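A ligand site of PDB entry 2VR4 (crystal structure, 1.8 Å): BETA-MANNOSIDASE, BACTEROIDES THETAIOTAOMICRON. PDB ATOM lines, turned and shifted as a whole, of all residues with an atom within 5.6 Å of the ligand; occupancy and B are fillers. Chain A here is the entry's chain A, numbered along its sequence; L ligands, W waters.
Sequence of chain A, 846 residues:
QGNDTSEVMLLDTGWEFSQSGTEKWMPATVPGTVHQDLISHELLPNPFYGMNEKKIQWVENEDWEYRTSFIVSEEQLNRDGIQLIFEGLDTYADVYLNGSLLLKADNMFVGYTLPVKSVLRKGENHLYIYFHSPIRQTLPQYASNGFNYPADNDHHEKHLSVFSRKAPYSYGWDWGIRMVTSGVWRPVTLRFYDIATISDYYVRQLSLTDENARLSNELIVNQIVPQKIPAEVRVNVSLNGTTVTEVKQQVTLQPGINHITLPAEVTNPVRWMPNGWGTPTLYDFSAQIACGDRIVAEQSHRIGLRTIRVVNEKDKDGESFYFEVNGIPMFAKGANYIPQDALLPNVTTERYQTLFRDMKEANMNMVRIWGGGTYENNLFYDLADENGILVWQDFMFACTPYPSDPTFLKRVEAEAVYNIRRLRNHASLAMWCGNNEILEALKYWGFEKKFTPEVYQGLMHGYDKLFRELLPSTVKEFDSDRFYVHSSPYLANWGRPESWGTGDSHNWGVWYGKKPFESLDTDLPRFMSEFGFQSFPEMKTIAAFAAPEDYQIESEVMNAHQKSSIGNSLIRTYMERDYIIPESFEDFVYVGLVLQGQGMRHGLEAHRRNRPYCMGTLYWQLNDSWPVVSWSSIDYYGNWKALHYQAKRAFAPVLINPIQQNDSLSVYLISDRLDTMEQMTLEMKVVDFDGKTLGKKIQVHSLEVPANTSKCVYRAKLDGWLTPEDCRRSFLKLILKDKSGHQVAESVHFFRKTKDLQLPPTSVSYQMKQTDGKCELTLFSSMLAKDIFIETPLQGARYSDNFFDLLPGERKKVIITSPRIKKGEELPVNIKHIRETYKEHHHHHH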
ATOM      1  N   ASN A 153      12.156   3.469  -9.693  1.00  0.00           N
ATOM      2  CA  ASN A 153      12.022   3.603 -11.139  1.00  0.00           C
ATOM      3  C   ASN A 153      12.732   4.824 -11.738  1.00  0.00           C
ATOM      4  O   ASN A 153      12.840   4.930 -12.947  1.00  0.00           O
ATOM      5  CB  ASN A 153      10.544   3.514 -11.565  1.00  0.00           C
ATOM      6  CG  ASN A 153       9.924   2.119 -11.310  1.00  0.00           C
ATOM      7  OD1 ASN A 153      10.207   1.188 -12.036  1.00  0.00           O
ATOM      8  ND2 ASN A 153       9.095   1.981 -10.271  1.00  0.00           N
ATOM      9  N   TRP A 173      11.632   3.852 -16.267  1.00  0.00           N
ATOM     10  CA  TRP A 173      10.668   2.999 -15.572  1.00  0.00           C
ATOM     11  C   TRP A 173      11.018   1.516 -15.876  1.00  0.00           C
ATOM     12  O   TRP A 173      11.962   1.262 -16.623  1.00  0.00           O
ATOM     13  CB  TRP A 173       9.211   3.326 -16.027  1.00  0.00           C
ATOM     14  CG  TRP A 173       8.230   3.044 -14.910  1.00  0.00           C
ATOM     15  CD1 TRP A 173       7.467   1.914 -14.753  1.00  0.00           C
ATOM     16  CD2 TRP A 173       7.923   3.887 -13.787  1.00  0.00           C
ATOM     17  NE1 TRP A 173       6.724   1.999 -13.613  1.00  0.00           N
ATOM     18  CE2 TRP A 173       6.973   3.201 -12.997  1.00  0.00           C
ATOM     19  CE3 TRP A 173       8.304   5.206 -13.405  1.00  0.00           C
ATOM     20  CZ2 TRP A 173       6.442   3.752 -11.819  1.00  0.00           C
ATOM     21  CZ3 TRP A 173       7.794   5.737 -12.227  1.00  0.00           C
ATOM     22  CH2 TRP A 173       6.872   5.009 -11.439  1.00  0.00           C
ATOM     23  N   ASP A 174      10.267   0.554 -15.345  1.00  0.00           N
ATOM     24  CA  ASP A 174      10.637  -0.866 -15.594  1.00  0.00           C
ATOM     25  C   ASP A 174      10.283  -1.424 -17.015  1.00  0.00           C
ATOM     26  O   ASP A 174      10.613  -2.585 -17.332  1.00  0.00           O
ATOM     27  CB  ASP A 174      10.246  -1.771 -14.435  1.00  0.00           C
ATOM     28  CG  ASP A 174       8.708  -1.788 -14.164  1.00  0.00           C
ATOM     29  OD1 ASP A 174       7.925  -1.369 -15.064  1.00  0.00           O
ATOM     30  OD2 ASP A 174       8.305  -2.227 -13.078  1.00  0.00           O
ATOM     31  N   TRP A 175       9.734  -0.580 -17.892  1.00  0.00           N
ATOM     32  CA  TRP A 175       9.566  -0.896 -19.360  1.00  0.00           C
ATOM     33  C   TRP A 175      10.027   0.252 -20.202  1.00  0.00           C
ATOM     34  O   TRP A 175       9.675   0.373 -21.386  1.00  0.00           O
ATOM     35  CB  TRP A 175       8.079  -1.174 -19.662  1.00  0.00           C
ATOM     36  CG  TRP A 175       7.160  -0.284 -18.837  1.00  0.00           C
ATOM     37  CD1 TRP A 175       6.430  -0.638 -17.779  1.00  0.00           C
ATOM     38  CD2 TRP A 175       6.978   1.152 -18.992  1.00  0.00           C
ATOM     39  NE1 TRP A 175       5.754   0.469 -17.261  1.00  0.00           N
ATOM     40  CE2 TRP A 175       6.071   1.563 -17.997  1.00  0.00           C
ATOM     41  CE3 TRP A 175       7.453   2.110 -19.917  1.00  0.00           C
ATOM     42  CZ2 TRP A 175       5.637   2.897 -17.868  1.00  0.00           C
ATOM     43  CZ3 TRP A 175       7.021   3.455 -19.769  1.00  0.00           C
ATOM     44  CH2 TRP A 175       6.139   3.821 -18.742  1.00  0.00           C
ATOM     45  N   ARG A 368      -7.354   2.399 -17.806  1.00  0.00           N
ATOM     46  CA  ARG A 368      -6.746   3.113 -16.697  1.00  0.00           C
ATOM     47  C   ARG A 368      -5.537   3.943 -17.190  1.00  0.00           C
ATOM     48  O   ARG A 368      -4.562   3.406 -17.727  1.00  0.00           O
ATOM     49  CB  ARG A 368      -6.382   2.167 -15.543  1.00  0.00           C
ATOM     50  CG  ARG A 368      -5.599   2.891 -14.426  1.00  0.00           C
ATOM     51  CD  ARG A 368      -5.452   2.082 -13.157  1.00  0.00           C
ATOM     52  NE  ARG A 368      -4.564   2.706 -12.188  1.00  0.00           N
ATOM     53  CZ  ARG A 368      -3.483   2.087 -11.637  1.00  0.00           C
ATOM     54  NH1 ARG A 368      -3.177   0.838 -11.971  1.00  0.00           N
ATOM     55  NH2 ARG A 368      -2.689   2.705 -10.740  1.00  0.00           N
ATOM     56  N   TRP A 370      -2.593   5.282 -16.084  1.00  0.00           N
ATOM     57  CA  TRP A 370      -1.770   5.023 -14.896  1.00  0.00           C
ATOM     58  C   TRP A 370      -0.893   6.220 -14.512  1.00  0.00           C
ATOM     59  O   TRP A 370      -0.396   6.950 -15.350  1.00  0.00           O
ATOM     60  CB  TRP A 370      -0.942   3.729 -15.131  1.00  0.00           C
ATOM     61  CG  TRP A 370       0.327   3.492 -14.354  1.00  0.00           C
ATOM     62  CD1 TRP A 370       0.479   2.723 -13.238  1.00  0.00           C
ATOM     63  CD2 TRP A 370       1.628   3.921 -14.738  1.00  0.00           C
ATOM     64  NE1 TRP A 370       1.808   2.725 -12.839  1.00  0.00           N
ATOM     65  CE2 TRP A 370       2.540   3.400 -13.781  1.00  0.00           C
ATOM     66  CE3 TRP A 370       2.122   4.674 -15.812  1.00  0.00           C
ATOM     67  CZ2 TRP A 370       3.894   3.658 -13.836  1.00  0.00           C
ATOM     68  CZ3 TRP A 370       3.477   4.924 -15.862  1.00  0.00           C
ATOM     69  CH2 TRP A 370       4.350   4.403 -14.890  1.00  0.00           C
ATOM     70  N   CYS A 399       4.292   5.062  -7.053  1.00  0.00           N
ATOM     71  CA  CYS A 399       5.235   4.137  -6.365  1.00  0.00           C
ATOM     72  C   CYS A 399       6.046   4.672  -5.196  1.00  0.00           C
ATOM     73  O   CYS A 399       6.353   3.939  -4.239  1.00  0.00           O
ATOM     74  CB  CYS A 399       6.129   3.421  -7.365  1.00  0.00           C
ATOM     75  SG  CYS A 399       5.203   2.485  -8.621  1.00  0.00           S
ATOM     76  N   ASN A 436      -0.665   5.591  -7.877  1.00  0.00           N
ATOM     77  CA  ASN A 436      -0.370   4.161  -8.033  1.00  0.00           C
ATOM     78  C   ASN A 436       0.573   3.659  -6.938  1.00  0.00           C
ATOM     79  O   ASN A 436       1.743   4.090  -6.871  1.00  0.00           O
ATOM     80  CB  ASN A 436       0.324   3.893  -9.378  1.00  0.00           C
ATOM     81  CG  ASN A 436       0.601   2.424  -9.592  1.00  0.00           C
ATOM     82  OD1 ASN A 436      -0.335   1.656  -9.794  1.00  0.00           O
ATOM     83  ND2 ASN A 436       1.896   2.017  -9.543  1.00  0.00           N
ATOM     84  N   GLU A 437       0.032   2.808  -6.047  1.00  0.00           N
ATOM     85  CA  GLU A 437       0.845   1.944  -5.147  1.00  0.00           C
ATOM     86  C   GLU A 437       1.648   2.661  -4.069  1.00  0.00           C
ATOM     87  O   GLU A 437       2.472   2.043  -3.398  1.00  0.00           O
ATOM     88  CB  GLU A 437       1.738   0.996  -5.979  1.00  0.00           C
ATOM     89  CG  GLU A 437       0.950  -0.066  -6.668  1.00  0.00           C
ATOM     90  CD  GLU A 437       1.824  -0.971  -7.579  1.00  0.00           C
ATOM     91  OE1 GLU A 437       3.027  -0.726  -7.775  1.00  0.00           O
ATOM     92  OE2 GLU A 437       1.236  -1.896  -8.156  1.00  0.00           O
ATOM     93  N   GLU A 440       0.762   1.181  -0.472  1.00  0.00           N
ATOM     94  CA  GLU A 440       1.395  -0.130  -0.444  1.00  0.00           C
ATOM     95  C   GLU A 440       2.899  -0.019  -0.246  1.00  0.00           C
ATOM     96  O   GLU A 440       3.486  -0.749   0.587  1.00  0.00           O
ATOM     97  CB  GLU A 440       1.145  -0.839  -1.781  1.00  0.00           C
ATOM     98  CG  GLU A 440       1.832  -2.185  -1.811  1.00  0.00           C
ATOM     99  CD  GLU A 440       1.407  -3.022  -2.977  1.00  0.00           C
ATOM    100  OE1 GLU A 440       0.348  -3.671  -2.913  1.00  0.00           O
ATOM    101  OE2 GLU A 440       2.170  -3.050  -3.970  1.00  0.00           O
ATOM    102  N   TRP A 445       7.031  -2.023   1.431  1.00  0.00           N
ATOM    103  CA  TRP A 445       8.125  -2.141   0.436  1.00  0.00           C
ATOM    104  C   TRP A 445       9.613  -2.198   0.893  1.00  0.00           C
ATOM    105  O   TRP A 445      10.485  -2.370   0.033  1.00  0.00           O
ATOM    106  CB  TRP A 445       7.918  -1.201  -0.788  1.00  0.00           C
ATOM    107  CG  TRP A 445       6.896  -1.729  -1.804  1.00  0.00           C
ATOM    108  CD1 TRP A 445       6.117  -2.845  -1.676  1.00  0.00           C
ATOM    109  CD2 TRP A 445       6.536  -1.127  -3.076  1.00  0.00           C
ATOM    110  NE1 TRP A 445       5.303  -2.992  -2.791  1.00  0.00           N
ATOM    111  CE2 TRP A 445       5.533  -1.956  -3.651  1.00  0.00           C
ATOM    112  CE3 TRP A 445       6.958   0.027  -3.774  1.00  0.00           C
ATOM    113  CZ2 TRP A 445       4.946  -1.670  -4.905  1.00  0.00           C
ATOM    114  CZ3 TRP A 445       6.378   0.311  -5.017  1.00  0.00           C
ATOM    115  CH2 TRP A 445       5.379  -0.536  -5.582  1.00  0.00           C
ATOM    116  N   TRP A 494      -1.159  -8.304  -2.613  1.00  0.00           N
ATOM    117  CA  TRP A 494      -1.163  -9.617  -3.269  1.00  0.00           C
ATOM    118  C   TRP A 494      -0.593 -10.729  -2.391  1.00  0.00           C
ATOM    119  O   TRP A 494      -0.863 -11.911  -2.669  1.00  0.00           O
ATOM    120  CB  TRP A 494      -0.480  -9.615  -4.638  1.00  0.00           C
ATOM    121  CG  TRP A 494       1.009  -9.337  -4.691  1.00  0.00           C
ATOM    122  CD1 TRP A 494       1.596  -8.143  -4.912  1.00  0.00           C
ATOM    123  CD2 TRP A 494       2.070 -10.307  -4.558  1.00  0.00           C
ATOM    124  NE1 TRP A 494       2.974  -8.285  -4.909  1.00  0.00           N
ATOM    125  CE2 TRP A 494       3.286  -9.603  -4.709  1.00  0.00           C
ATOM    126  CE3 TRP A 494       2.110 -11.689  -4.339  1.00  0.00           C
ATOM    127  CZ2 TRP A 494       4.542 -10.249  -4.665  1.00  0.00           C
ATOM    128  CZ3 TRP A 494       3.355 -12.327  -4.278  1.00  0.00           C
ATOM    129  CH2 TRP A 494       4.556 -11.597  -4.438  1.00  0.00           C
ATOM    130  N   HIS A 506      -3.936  -5.260  -7.177  1.00  0.00           N
ATOM    131  CA  HIS A 506      -2.861  -5.470  -8.160  1.00  0.00           C
ATOM    132  C   HIS A 506      -2.236  -6.830  -7.853  1.00  0.00           C
ATOM    133  O   HIS A 506      -1.319  -6.917  -7.046  1.00  0.00           O
ATOM    134  CB  HIS A 506      -1.759  -4.390  -8.017  1.00  0.00           C
ATOM    135  CG  HIS A 506      -2.235  -2.994  -8.361  1.00  0.00           C
ATOM    136  ND1 HIS A 506      -1.374  -1.924  -8.499  1.00  0.00           N
ATOM    137  CD2 HIS A 506      -3.485  -2.492  -8.548  1.00  0.00           C
ATOM    138  CE1 HIS A 506      -2.067  -0.825  -8.759  1.00  0.00           C
ATOM    139  NE2 HIS A 506      -3.354  -1.144  -8.810  1.00  0.00           N
ATOM    140  N   TRP A 508       0.157  -9.208  -8.319  1.00  0.00           N
ATOM    141  CA  TRP A 508       1.460  -9.467  -8.876  1.00  0.00           C
ATOM    142  C   TRP A 508       2.078 -10.788  -8.343  1.00  0.00           C
ATOM    143  O   TRP A 508       3.267 -10.994  -8.414  1.00  0.00           O
ATOM    144  CB  TRP A 508       2.387  -8.240  -8.759  1.00  0.00           C
ATOM    145  CG  TRP A 508       1.959  -7.169  -9.741  1.00  0.00           C
ATOM    146  CD1 TRP A 508       1.237  -6.043  -9.470  1.00  0.00           C
ATOM    147  CD2 TRP A 508       2.218  -7.176 -11.137  1.00  0.00           C
ATOM    148  NE1 TRP A 508       1.019  -5.323 -10.660  1.00  0.00           N
ATOM    149  CE2 TRP A 508       1.602  -6.008 -11.686  1.00  0.00           C
ATOM    150  CE3 TRP A 508       2.865  -8.087 -11.990  1.00  0.00           C
ATOM    151  CZ2 TRP A 508       1.687  -5.693 -13.055  1.00  0.00           C
ATOM    152  CZ3 TRP A 508       2.960  -7.783 -13.359  1.00  0.00           C
ATOM    153  CH2 TRP A 508       2.365  -6.593 -13.881  1.00  0.00           C
ATOM    154  N   TYR A 512       5.796 -11.434 -10.458  1.00  0.00           N
ATOM    155  CA  TYR A 512       6.686 -11.135  -9.298  1.00  0.00           C
ATOM    156  C   TYR A 512       6.701 -12.245  -8.241  1.00  0.00           C
ATOM    157  O   TYR A 512       7.778 -12.567  -7.710  1.00  0.00           O
ATOM    158  CB  TYR A 512       6.360  -9.803  -8.601  1.00  0.00           C
ATOM    159  CG  TYR A 512       6.754  -8.675  -9.450  1.00  0.00           C
ATOM    160  CD1 TYR A 512       8.102  -8.408  -9.684  1.00  0.00           C
ATOM    161  CD2 TYR A 512       5.795  -7.903 -10.109  1.00  0.00           C
ATOM    162  CE1 TYR A 512       8.485  -7.395 -10.523  1.00  0.00           C
ATOM    163  CE2 TYR A 512       6.188  -6.838 -10.982  1.00  0.00           C
ATOM    164  CZ  TYR A 512       7.536  -6.613 -11.169  1.00  0.00           C
ATOM    165  OH  TYR A 512       7.963  -5.615 -12.029  1.00  0.00           O
ATOM    166  N   GLU A 530      -4.720  -4.380 -11.778  1.00  0.00           N
ATOM    167  CA  GLU A 530      -3.492  -4.756 -12.482  1.00  0.00           C
ATOM    168  C   GLU A 530      -3.239  -6.252 -12.276  1.00  0.00           C
ATOM    169  O   GLU A 530      -3.375  -6.728 -11.156  1.00  0.00           O
ATOM    170  CB  GLU A 530      -2.240  -4.086 -11.853  1.00  0.00           C
ATOM    171  CG  GLU A 530      -2.201  -2.520 -11.936  1.00  0.00           C
ATOM    172  CD  GLU A 530      -0.802  -1.962 -11.668  1.00  0.00           C
ATOM    173  OE1 GLU A 530       0.129  -2.785 -11.419  1.00  0.00           O
ATOM    174  OE2 GLU A 530      -0.629  -0.720 -11.689  1.00  0.00           O
ATOM    175  N   SER A 564      12.513  -4.936 -15.328  1.00  0.00           N
ATOM    176  CA  SER A 564      11.846  -5.473 -14.145  1.00  0.00           C
ATOM    177  C   SER A 564      12.872  -6.141 -13.218  1.00  0.00           C
ATOM    178  O   SER A 564      13.883  -6.693 -13.696  1.00  0.00           O
ATOM    179  CB  SER A 564      10.760  -6.479 -14.565  1.00  0.00           C
ATOM    180  OG  SER A 564      10.182  -7.159 -13.454  1.00  0.00           O
ATOM    181  N   TRP A 620      -2.179  -5.356 -16.891  1.00  0.00           N
ATOM    182  CA  TRP A 620      -0.941  -4.596 -17.057  1.00  0.00           C
ATOM    183  C   TRP A 620      -0.157  -5.280 -18.218  1.00  0.00           C
ATOM    184  O   TRP A 620       0.271  -6.412 -18.029  1.00  0.00           O
ATOM    185  CB  TRP A 620      -0.105  -4.597 -15.740  1.00  0.00           C
ATOM    186  CG  TRP A 620       1.021  -3.667 -15.955  1.00  0.00           C
ATOM    187  CD1 TRP A 620       2.241  -3.919 -16.587  1.00  0.00           C
ATOM    188  CD2 TRP A 620       0.943  -2.241 -15.811  1.00  0.00           C
ATOM    189  NE1 TRP A 620       2.955  -2.726 -16.741  1.00  0.00           N
ATOM    190  CE2 TRP A 620       2.172  -1.692 -16.263  1.00  0.00           C
ATOM    191  CE3 TRP A 620      -0.032  -1.383 -15.274  1.00  0.00           C
ATOM    192  CZ2 TRP A 620       2.427  -0.290 -16.248  1.00  0.00           C
ATOM    193  CZ3 TRP A 620       0.241  -0.005 -15.225  1.00  0.00           C
ATOM    194  CH2 TRP A 620       1.437   0.522 -15.723  1.00  0.00           C
ATOM    195  N   GLN A 621       0.038  -4.657 -19.394  1.00  0.00           N
ATOM    196  CA  GLN A 621      -0.259  -3.266 -19.737  1.00  0.00           C
ATOM    197  C   GLN A 621      -0.727  -3.325 -21.194  1.00  0.00           C
ATOM    198  O   GLN A 621      -0.480  -4.335 -21.920  1.00  0.00           O
ATOM    199  CB  GLN A 621       1.036  -2.391 -19.653  1.00  0.00           C
ATOM    200  CG  GLN A 621       2.099  -2.591 -20.752  1.00  0.00           C
ATOM    201  CD  GLN A 621       3.511  -2.171 -20.284  1.00  0.00           C
ATOM    202  OE1 GLN A 621       4.110  -2.827 -19.430  1.00  0.00           O
ATOM    203  NE2 GLN A 621       4.046  -1.116 -20.873  1.00  0.00           N
ATOM    204  N   TRP A 631       5.315  -6.077 -20.489  1.00  0.00           N
ATOM    205  CA  TRP A 631       4.030  -6.712 -20.238  1.00  0.00           C
ATOM    206  C   TRP A 631       2.958  -6.331 -21.245  1.00  0.00           C
ATOM    207  O   TRP A 631       1.815  -6.718 -21.072  1.00  0.00           O
ATOM    208  CB  TRP A 631       3.537  -6.293 -18.838  1.00  0.00           C
ATOM    209  CG  TRP A 631       4.503  -6.657 -17.720  1.00  0.00           C
ATOM    210  CD1 TRP A 631       4.398  -7.703 -16.887  1.00  0.00           C
ATOM    211  CD2 TRP A 631       5.690  -5.946 -17.353  1.00  0.00           C
ATOM    212  NE1 TRP A 631       5.472  -7.727 -15.997  1.00  0.00           N
ATOM    213  CE2 TRP A 631       6.285  -6.664 -16.285  1.00  0.00           C
ATOM    214  CE3 TRP A 631       6.319  -4.774 -17.824  1.00  0.00           C
ATOM    215  CZ2 TRP A 631       7.481  -6.230 -15.651  1.00  0.00           C
ATOM    216  CZ3 TRP A 631       7.521  -4.353 -17.214  1.00  0.00           C
ATOM    217  CH2 TRP A 631       8.085  -5.094 -16.133  1.00  0.00           C
HETATM  218  C1  LIG L   1       5.479  -4.812  -8.195  1.00  0.00           C
HETATM  219  C2  LIG L   1       2.620  -1.043 -12.156  1.00  0.00           C
HETATM  220  C3  LIG L   1       3.740  -0.280 -12.943  1.00  0.00           C
HETATM  221  C4  LIG L   1       4.848  -1.233 -13.491  1.00  0.00           C
HETATM  222  C5  LIG L   1       4.317  -2.690 -13.609  1.00  0.00           C
HETATM  223  C6  LIG L   1       5.293  -3.732 -14.195  1.00  0.00           C
HETATM  224  O1  LIG L   1       1.864  -0.367 -11.156  1.00  0.00           O
HETATM  225  O2  LIG L   1       4.298   0.677 -12.044  1.00  0.00           O
HETATM  226  O3  LIG L   1       5.373  -0.773 -14.729  1.00  0.00           O
HETATM  227  N1  LIG L   1       3.877  -3.132 -12.317  1.00  0.00           N
HETATM  228  O4  LIG L   1       6.328  -3.997 -13.236  1.00  0.00           O
HETATM  229  N2  LIG L   1       7.028  -4.492  -6.265  1.00  0.00           N
HETATM  230  C7  LIG L   1       6.938  -4.755  -7.716  1.00  0.00           C
HETATM  231  C8  LIG L   1       3.558  -3.727  -9.465  1.00  0.00           C
HETATM  232  C9  LIG L   1       4.994  -3.561  -8.934  1.00  0.00           C
HETATM  233  N3  LIG L   1       3.052  -2.580 -10.211  1.00  0.00           N
HETATM  234  C10 LIG L   1       3.237  -2.327 -11.503  1.00  0.00           C
HETATM  235  O   HOH W   1       5.138  -0.486  -9.695  1.00  0.00           O
HETATM  236  O   HOH W   2       5.713  -7.027  -5.500  1.00  0.00           O
HETATM  237  O   HOH W   3      10.122  -5.124  -7.937  1.00  0.00           O
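Water W1 lies within hydrogen-bond range of an oxygen (O2) of the ligand (2.8 Å), the side-chain carboxylate (OE1) of Glu 437 (2.9 Å) and the side-chain sulfur (SG) of Cys 399 (3.2 Å).
Water W2 lies within hydrogen-bond range of a nitrogen (N2) of the ligand (3.0 Å) and the indole nitrogen of Trp 494 (3.1 Å).
NE1 of Trp 173 sits at hydrogen-bond distance from O2 of the ligand, 3.2 Å away.
NE1 of Trp 175 is in hydrogen-bond range of O3 of the ligand (2.8 Å).
NE1 of Trp 370 sits at hydrogen-bond distance from O2 of the ligand.
NE1 of Trp 508 sits close to N3 of the ligand.
The side-chain carboxylate (OE2) of Glu 530 lies within hydrogen-bond range of an oxygen (O1) of the ligand (2.6 Å).
An oxygen (O4) of the ligand sits at hydrogen-bond distance from the side-chain hydroxyl (OH) of Tyr 512.
The side-chain carboxylate (OD1) of Asp 174 is in hydrogen-bond range of an oxygen (O3) of the ligand (2.6 Å).
OE2 of Glu 437 sits close to O1 of the ligand, at 3.4 Å.
An oxygen (O1) of the ligand sits at hydrogen-bond distance from the side-chain amide nitrogen of Asn 436 (2.9 Å).
ND1 of His 506 lies within hydrogen-bond range of OE2 of Glu 437 (2.6 Å).
OE1 of Glu 530 is in hydrogen-bond range of NE1 of Trp 508.
The guanidinium group (NH2) of Arg 368 is in hydrogen-bond range of the side-chain amide oxygen (OD1) of Asn 436.
The side-chain hydroxyl of Tyr 512 lies within hydrogen-bond range of the side-chain hydroxyl of Ser 564, at 3.1 Å.
The backbone NH of Gln 621 is in hydrogen-bond range of the backbone carbonyl oxygen of Trp 631, at 3.2 Å.
The side-chain amide nitrogen of Asn 436 lies close to the indole nitrogen of Trp 370 (3.4 Å).
The backbone NH of Asp 174 is in hydrogen-bond range of the side-chain amide oxygen of Asn 153 (3.4 Å).
OD1 of Asn 436 sits close to OE2 of Glu 530 (3.1 Å).
Residues that only touch the ligand: Trp 620, Trp 631, Trp 445 and Cys 399.
Hydrophobic or aromatic side chains that line the ligand: Trp 173, Trp 175, Trp 370, Trp 445, Trp 508, Tyr 512, Trp 620 and Trp 631.
Of the 20 residues printed, 13 come within 4 Å of the ligand.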
